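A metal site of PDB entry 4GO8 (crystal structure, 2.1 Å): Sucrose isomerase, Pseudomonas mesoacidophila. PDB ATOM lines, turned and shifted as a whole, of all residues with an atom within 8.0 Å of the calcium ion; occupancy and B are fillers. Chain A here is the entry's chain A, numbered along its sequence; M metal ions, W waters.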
ATOM      1  N   PRO A  17      24.357 -10.233  27.867  1.00  0.00           N
ATOM      2  CA  PRO A  17      23.602 -10.764  26.727  1.00  0.00           C
ATOM      3  C   PRO A  17      24.342 -10.690  25.407  1.00  0.00           C
ATOM      4  O   PRO A  17      24.166 -11.556  24.566  1.00  0.00           O
ATOM      5  CB  PRO A  17      22.360  -9.866  26.685  1.00  0.00           C
ATOM      6  CG  PRO A  17      22.232  -9.337  28.079  1.00  0.00           C
ATOM      7  CD  PRO A  17      23.641  -9.137  28.534  1.00  0.00           C
ATOM      8  N   ARG A  18      25.171  -9.662  25.243  1.00  0.00           N
ATOM      9  CA  ARG A  18      25.970  -9.495  24.033  1.00  0.00           C
ATOM     10  C   ARG A  18      26.890 -10.687  23.780  1.00  0.00           C
ATOM     11  O   ARG A  18      27.194 -11.013  22.637  1.00  0.00           O
ATOM     12  CB  ARG A  18      26.794  -8.198  24.119  1.00  0.00           C
ATOM     13  CG  ARG A  18      27.540  -7.833  22.848  1.00  0.00           C
ATOM     14  CD  ARG A  18      28.236  -6.483  22.973  1.00  0.00           C
ATOM     15  NE  ARG A  18      28.871  -6.090  21.713  1.00  0.00           N
ATOM     16  CZ  ARG A  18      28.276  -5.364  20.768  1.00  0.00           C
ATOM     17  NH1 ARG A  18      27.030  -4.942  20.933  1.00  0.00           N
ATOM     18  NH2 ARG A  18      28.926  -5.059  19.659  1.00  0.00           N
ATOM     19  N   LYS A  21      24.555 -15.852  24.273  1.00  0.00           N
ATOM     20  CA  LYS A  21      24.129 -16.783  23.226  1.00  0.00           C
ATOM     21  C   LYS A  21      23.455 -16.124  22.027  1.00  0.00           C
ATOM     22  O   LYS A  21      22.434 -15.438  22.170  1.00  0.00           O
ATOM     23  CB  LYS A  21      23.218 -17.866  23.799  1.00  0.00           C
ATOM     24  CG  LYS A  21      22.782 -18.902  22.764  1.00  0.00           C
ATOM     25  CD  LYS A  21      23.961 -19.728  22.276  1.00  0.00           C
ATOM     26  CE  LYS A  21      23.650 -20.407  20.950  1.00  0.00           C
ATOM     27  NZ  LYS A  21      22.419 -21.231  21.005  1.00  0.00           N
ATOM     28  N   ASP A  22      24.026 -16.338  20.841  1.00  0.00           N
ATOM     29  CA  ASP A  22      23.476 -15.803  19.588  1.00  0.00           C
ATOM     30  C   ASP A  22      22.566 -16.832  18.919  1.00  0.00           C
ATOM     31  O   ASP A  22      22.871 -18.022  18.891  1.00  0.00           O
ATOM     32  CB  ASP A  22      24.637 -15.419  18.657  1.00  0.00           C
ATOM     33  CG  ASP A  22      24.164 -14.859  17.329  1.00  0.00           C
ATOM     34  OD1 ASP A  22      23.013 -14.387  17.250  1.00  0.00           O
ATOM     35  OD2 ASP A  22      24.963 -14.863  16.364  1.00  0.00           O
ATOM     36  N   THR A  23      21.424 -16.378  18.381  1.00  0.00           N
ATOM     37  CA  THR A  23      20.477 -17.291  17.742  1.00  0.00           C
ATOM     38  C   THR A  23      20.137 -16.947  16.295  1.00  0.00           C
ATOM     39  O   THR A  23      19.275 -17.595  15.698  1.00  0.00           O
ATOM     40  CB  THR A  23      19.158 -17.418  18.535  1.00  0.00           C
ATOM     41  OG1 THR A  23      18.563 -16.120  18.716  1.00  0.00           O
ATOM     42  CG2 THR A  23      19.388 -18.063  19.881  1.00  0.00           C
ATOM     43  N   ASN A  24      20.782 -15.937  15.716  1.00  0.00           N
ATOM     44  CA  ASN A  24      20.513 -15.583  14.325  1.00  0.00           C
ATOM     45  C   ASN A  24      21.781 -15.317  13.510  1.00  0.00           C
ATOM     46  O   ASN A  24      21.705 -14.750  12.414  1.00  0.00           O
ATOM     47  CB  ASN A  24      19.555 -14.388  14.244  1.00  0.00           C
ATOM     48  CG  ASN A  24      20.162 -13.112  14.776  1.00  0.00           C
ATOM     49  OD1 ASN A  24      21.063 -13.153  15.616  1.00  0.00           O
ATOM     50  ND2 ASN A  24      19.675 -11.973  14.306  1.00  0.00           N
ATOM     51  N   GLY A  25      22.921 -15.726  14.039  1.00  0.00           N
ATOM     52  CA  GLY A  25      24.178 -15.671  13.312  1.00  0.00           C
ATOM     53  C   GLY A  25      24.759 -14.301  13.027  1.00  0.00           C
ATOM     54  O   GLY A  25      25.627 -14.162  12.166  1.00  0.00           O
ATOM     55  N   ASP A  26      24.292 -13.279  13.728  1.00  0.00           N
ATOM     56  CA  ASP A  26      24.824 -11.936  13.534  1.00  0.00           C
ATOM     57  C   ASP A  26      26.068 -11.697  14.398  1.00  0.00           C
ATOM     58  O   ASP A  26      26.688 -10.628  14.338  1.00  0.00           O
ATOM     59  CB  ASP A  26      23.761 -10.863  13.783  1.00  0.00           C
ATOM     60  CG  ASP A  26      23.413 -10.701  15.245  1.00  0.00           C
ATOM     61  OD1 ASP A  26      23.634 -11.656  16.030  1.00  0.00           O
ATOM     62  OD2 ASP A  26      22.918  -9.617  15.628  1.00  0.00           O
ATOM     63  N   GLY A  27      26.421 -12.692  15.207  1.00  0.00           N
ATOM     64  CA  GLY A  27      27.609 -12.611  16.040  1.00  0.00           C
ATOM     65  C   GLY A  27      27.371 -11.947  17.369  1.00  0.00           C
ATOM     66  O   GLY A  27      28.286 -11.819  18.191  1.00  0.00           O
ATOM     67  N   ILE A  28      26.132 -11.504  17.598  1.00  0.00           N
ATOM     68  CA  ILE A  28      25.782 -10.854  18.852  1.00  0.00           C
ATOM     69  C   ILE A  28      24.708 -11.664  19.593  1.00  0.00           C
ATOM     70  O   ILE A  28      23.715 -12.060  18.994  1.00  0.00           O
ATOM     71  CB  ILE A  28      25.274  -9.415  18.610  1.00  0.00           C
ATOM     72  CG1 ILE A  28      26.382  -8.579  17.980  1.00  0.00           C
ATOM     73  CG2 ILE A  28      24.798  -8.789  19.909  1.00  0.00           C
ATOM     74  CD1 ILE A  28      25.959  -7.158  17.641  1.00  0.00           C
ATOM     75  N   GLY A  29      24.926 -11.889  20.879  1.00  0.00           N
ATOM     76  CA  GLY A  29      23.956 -12.595  21.687  1.00  0.00           C
ATOM     77  C   GLY A  29      22.650 -11.831  21.778  1.00  0.00           C
ATOM     78  O   GLY A  29      22.612 -10.613  21.585  1.00  0.00           O
ATOM     79  N   ASP A  30      21.572 -12.548  22.063  1.00  0.00           N
ATOM     80  CA  ASP A  30      20.235 -11.964  22.056  1.00  0.00           C
ATOM     81  C   ASP A  30      19.330 -12.578  23.127  1.00  0.00           C
ATOM     82  O   ASP A  30      19.740 -13.496  23.840  1.00  0.00           O
ATOM     83  CB  ASP A  30      19.601 -12.154  20.673  1.00  0.00           C
ATOM     84  CG  ASP A  30      19.865 -13.527  20.105  1.00  0.00           C
ATOM     85  OD1 ASP A  30      19.277 -14.505  20.616  1.00  0.00           O
ATOM     86  OD2 ASP A  30      20.654 -13.636  19.153  1.00  0.00           O
ATOM     87  N   PHE A  31      18.108 -12.070  23.220  1.00  0.00           N
ATOM     88  CA  PHE A  31      17.142 -12.544  24.206  1.00  0.00           C
ATOM     89  C   PHE A  31      16.752 -14.006  24.013  1.00  0.00           C
ATOM     90  O   PHE A  31      16.628 -14.753  24.987  1.00  0.00           O
ATOM     91  CB  PHE A  31      15.894 -11.671  24.202  1.00  0.00           C
ATOM     92  CG  PHE A  31      16.028 -10.421  25.016  1.00  0.00           C
ATOM     93  CD1 PHE A  31      16.715 -10.430  26.214  1.00  0.00           C
ATOM     94  CD2 PHE A  31      15.470  -9.228  24.576  1.00  0.00           C
ATOM     95  CE1 PHE A  31      16.841  -9.287  26.959  1.00  0.00           C
ATOM     96  CE2 PHE A  31      15.594  -8.085  25.330  1.00  0.00           C
ATOM     97  CZ  PHE A  31      16.280  -8.103  26.517  1.00  0.00           C
ATOM     98  N   LYS A  32      16.527 -14.395  22.771  1.00  0.00           N
ATOM     99  CA  LYS A  32      16.181 -15.772  22.450  1.00  0.00           C
ATOM    100  C   LYS A  32      17.284 -16.726  22.910  1.00  0.00           C
ATOM    101  O   LYS A  32      17.005 -17.823  23.383  1.00  0.00           O
ATOM    102  CB  LYS A  32      15.927 -15.934  20.950  1.00  0.00           C
ATOM    103  N   GLY A  33      18.528 -16.294  22.784  1.00  0.00           N
ATOM    104  CA  GLY A  33      19.667 -17.078  23.230  1.00  0.00           C
ATOM    105  C   GLY A  33      19.657 -17.322  24.726  1.00  0.00           C
ATOM    106  O   GLY A  33      19.895 -18.434  25.189  1.00  0.00           O
ATOM    107  N   LYS A  74      17.829  -3.324  19.657  1.00  0.00           N
ATOM    108  CA  LYS A  74      17.520  -4.015  18.412  1.00  0.00           C
ATOM    109  C   LYS A  74      18.251  -5.358  18.286  1.00  0.00           C
ATOM    110  O   LYS A  74      17.669  -6.341  17.827  1.00  0.00           O
ATOM    111  CB  LYS A  74      17.847  -3.130  17.211  1.00  0.00           C
ATOM    112  N   GLU A  75      19.514  -5.389  18.698  1.00  0.00           N
ATOM    113  CA  GLU A  75      20.321  -6.603  18.605  1.00  0.00           C
ATOM    114  C   GLU A  75      19.792  -7.737  19.486  1.00  0.00           C
ATOM    115  O   GLU A  75      19.931  -8.911  19.139  1.00  0.00           O
ATOM    116  CB  GLU A  75      21.786  -6.304  18.964  1.00  0.00           C
ATOM    117  CG  GLU A  75      22.569  -5.559  17.886  1.00  0.00           C
ATOM    118  CD  GLU A  75      22.267  -4.074  17.861  1.00  0.00           C
ATOM    119  OE1 GLU A  75      21.752  -3.545  18.862  1.00  0.00           O
ATOM    120  OE2 GLU A  75      22.561  -3.424  16.824  1.00  0.00           O
ATOM    121  N   TYR A  76      19.181  -7.394  20.620  1.00  0.00           N
ATOM    122  CA  TYR A  76      18.716  -8.420  21.561  1.00  0.00           C
ATOM    123  C   TYR A  76      17.341  -8.965  21.195  1.00  0.00           C
ATOM    124  O   TYR A  76      17.002 -10.100  21.552  1.00  0.00           O
ATOM    125  CB  TYR A  76      18.726  -7.881  22.993  1.00  0.00           C
ATOM    126  CG  TYR A  76      20.092  -7.490  23.502  1.00  0.00           C
ATOM    127  CD1 TYR A  76      21.247  -7.875  22.820  1.00  0.00           C
ATOM    128  CD2 TYR A  76      20.246  -6.732  24.659  1.00  0.00           C
ATOM    129  CE1 TYR A  76      22.499  -7.522  23.274  1.00  0.00           C
ATOM    130  CE2 TYR A  76      21.497  -6.379  25.122  1.00  0.00           C
ATOM    131  CZ  TYR A  76      22.620  -6.772  24.423  1.00  0.00           C
ATOM    132  OH  TYR A  76      23.872  -6.418  24.877  1.00  0.00           O
ATOM    133  N   GLY A  77      16.555  -8.179  20.481  1.00  0.00           N
ATOM    134  CA  GLY A  77      15.225  -8.605  20.060  1.00  0.00           C
ATOM    135  C   GLY A  77      14.187  -7.516  20.202  1.00  0.00           C
ATOM    136  O   GLY A  77      14.506  -6.327  20.140  1.00  0.00           O
ATOM    137  N   PHE A 431      28.636 -20.504  20.434  1.00  0.00           N
ATOM    138  CA  PHE A 431      28.033 -19.208  20.726  1.00  0.00           C
ATOM    139  C   PHE A 431      27.255 -18.673  19.530  1.00  0.00           C
ATOM    140  O   PHE A 431      26.153 -18.140  19.679  1.00  0.00           O
ATOM    141  CB  PHE A 431      29.100 -18.193  21.150  1.00  0.00           C
ATOM    142  CG  PHE A 431      28.639 -16.759  21.060  1.00  0.00           C
ATOM    143  CD1 PHE A 431      27.777 -16.225  22.002  1.00  0.00           C
ATOM    144  CD2 PHE A 431      29.094 -15.935  20.044  1.00  0.00           C
ATOM    145  CE1 PHE A 431      27.354 -14.913  21.922  1.00  0.00           C
ATOM    146  CE2 PHE A 431      28.685 -14.617  19.957  1.00  0.00           C
ATOM    147  CZ  PHE A 431      27.816 -14.101  20.897  1.00  0.00           C
ATOM    148  N   THR A 432      27.839 -18.796  18.353  1.00  0.00           N
ATOM    149  CA  THR A 432      27.216 -18.293  17.135  1.00  0.00           C
ATOM    150  C   THR A 432      27.555 -19.149  15.927  1.00  0.00           C
ATOM    151  O   THR A 432      28.551 -19.887  15.929  1.00  0.00           O
ATOM    152  CB  THR A 432      27.645 -16.836  16.855  1.00  0.00           C
ATOM    153  OG1 THR A 432      26.954 -16.338  15.704  1.00  0.00           O
ATOM    154  CG2 THR A 432      29.141 -16.768  16.594  1.00  0.00           C
HETATM  155 CA    CA M   1      21.944 -12.307  17.525  1.00  0.00          CA
HETATM  156  O   HOH W   1      19.801 -11.023  17.276  1.00  0.00           O
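OD2 of Asp 22 sits at hydrogen-bond distance from N of Gly 25, 3.2 Å away. OD2 of Asp 22 is in hydrogen-bond range of N of Gly 27, 2.9 Å away. OD2 of Asp 22 sits at hydrogen-bond distance from OG1 of Thr 432, 2.6 Å away. The backbone carbonyl oxygen of Phe 431 sits at hydrogen-bond distance from the backbone NH of Asp 22, at 3.0 Å. OD1 of Asp 30 sits at hydrogen-bond distance from OG1 of Thr 23. N of Asp 30 lies within hydrogen-bond range of O of Lys 21. The backbone NH (N) of Gly 33 lies within hydrogen-bond range of the side-chain carboxylate (OD1) of Asp 30. N of Lys 32 lies close to OD1 of Asp 30.
Within 4 Å of the calcium ion: Asp 22, Asn 24, Asp 26, Ile 28 and Asp 30. The nearest printed residue that does not touch the calcium ion is Thr 23 (4.2 Å).
The calcium ion is bound by the side-chain amide oxygen (OD1) of Asn 24 (2.3 Å), the backbone carbonyl oxygen (O) of Ile 28 (2.3 Å), the side-chain carboxylate (OD1) of Asp 26 (2.3 Å), the side-chain carboxylate (OD1) of Asp 22 (2.4 Å), the side-chain carboxylate (OD2) of Asp 30 (2.5 Å) and water W1 (2.5 Å). The calcium ion has six donor atoms within binding distance.
Water W1 lies within hydrogen-bond range of the backbone carbonyl oxygen (O) of Glu 75 (2.8 Å) and the side-chain amide nitrogen (ND2) of Asn 24 (3.1 Å).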
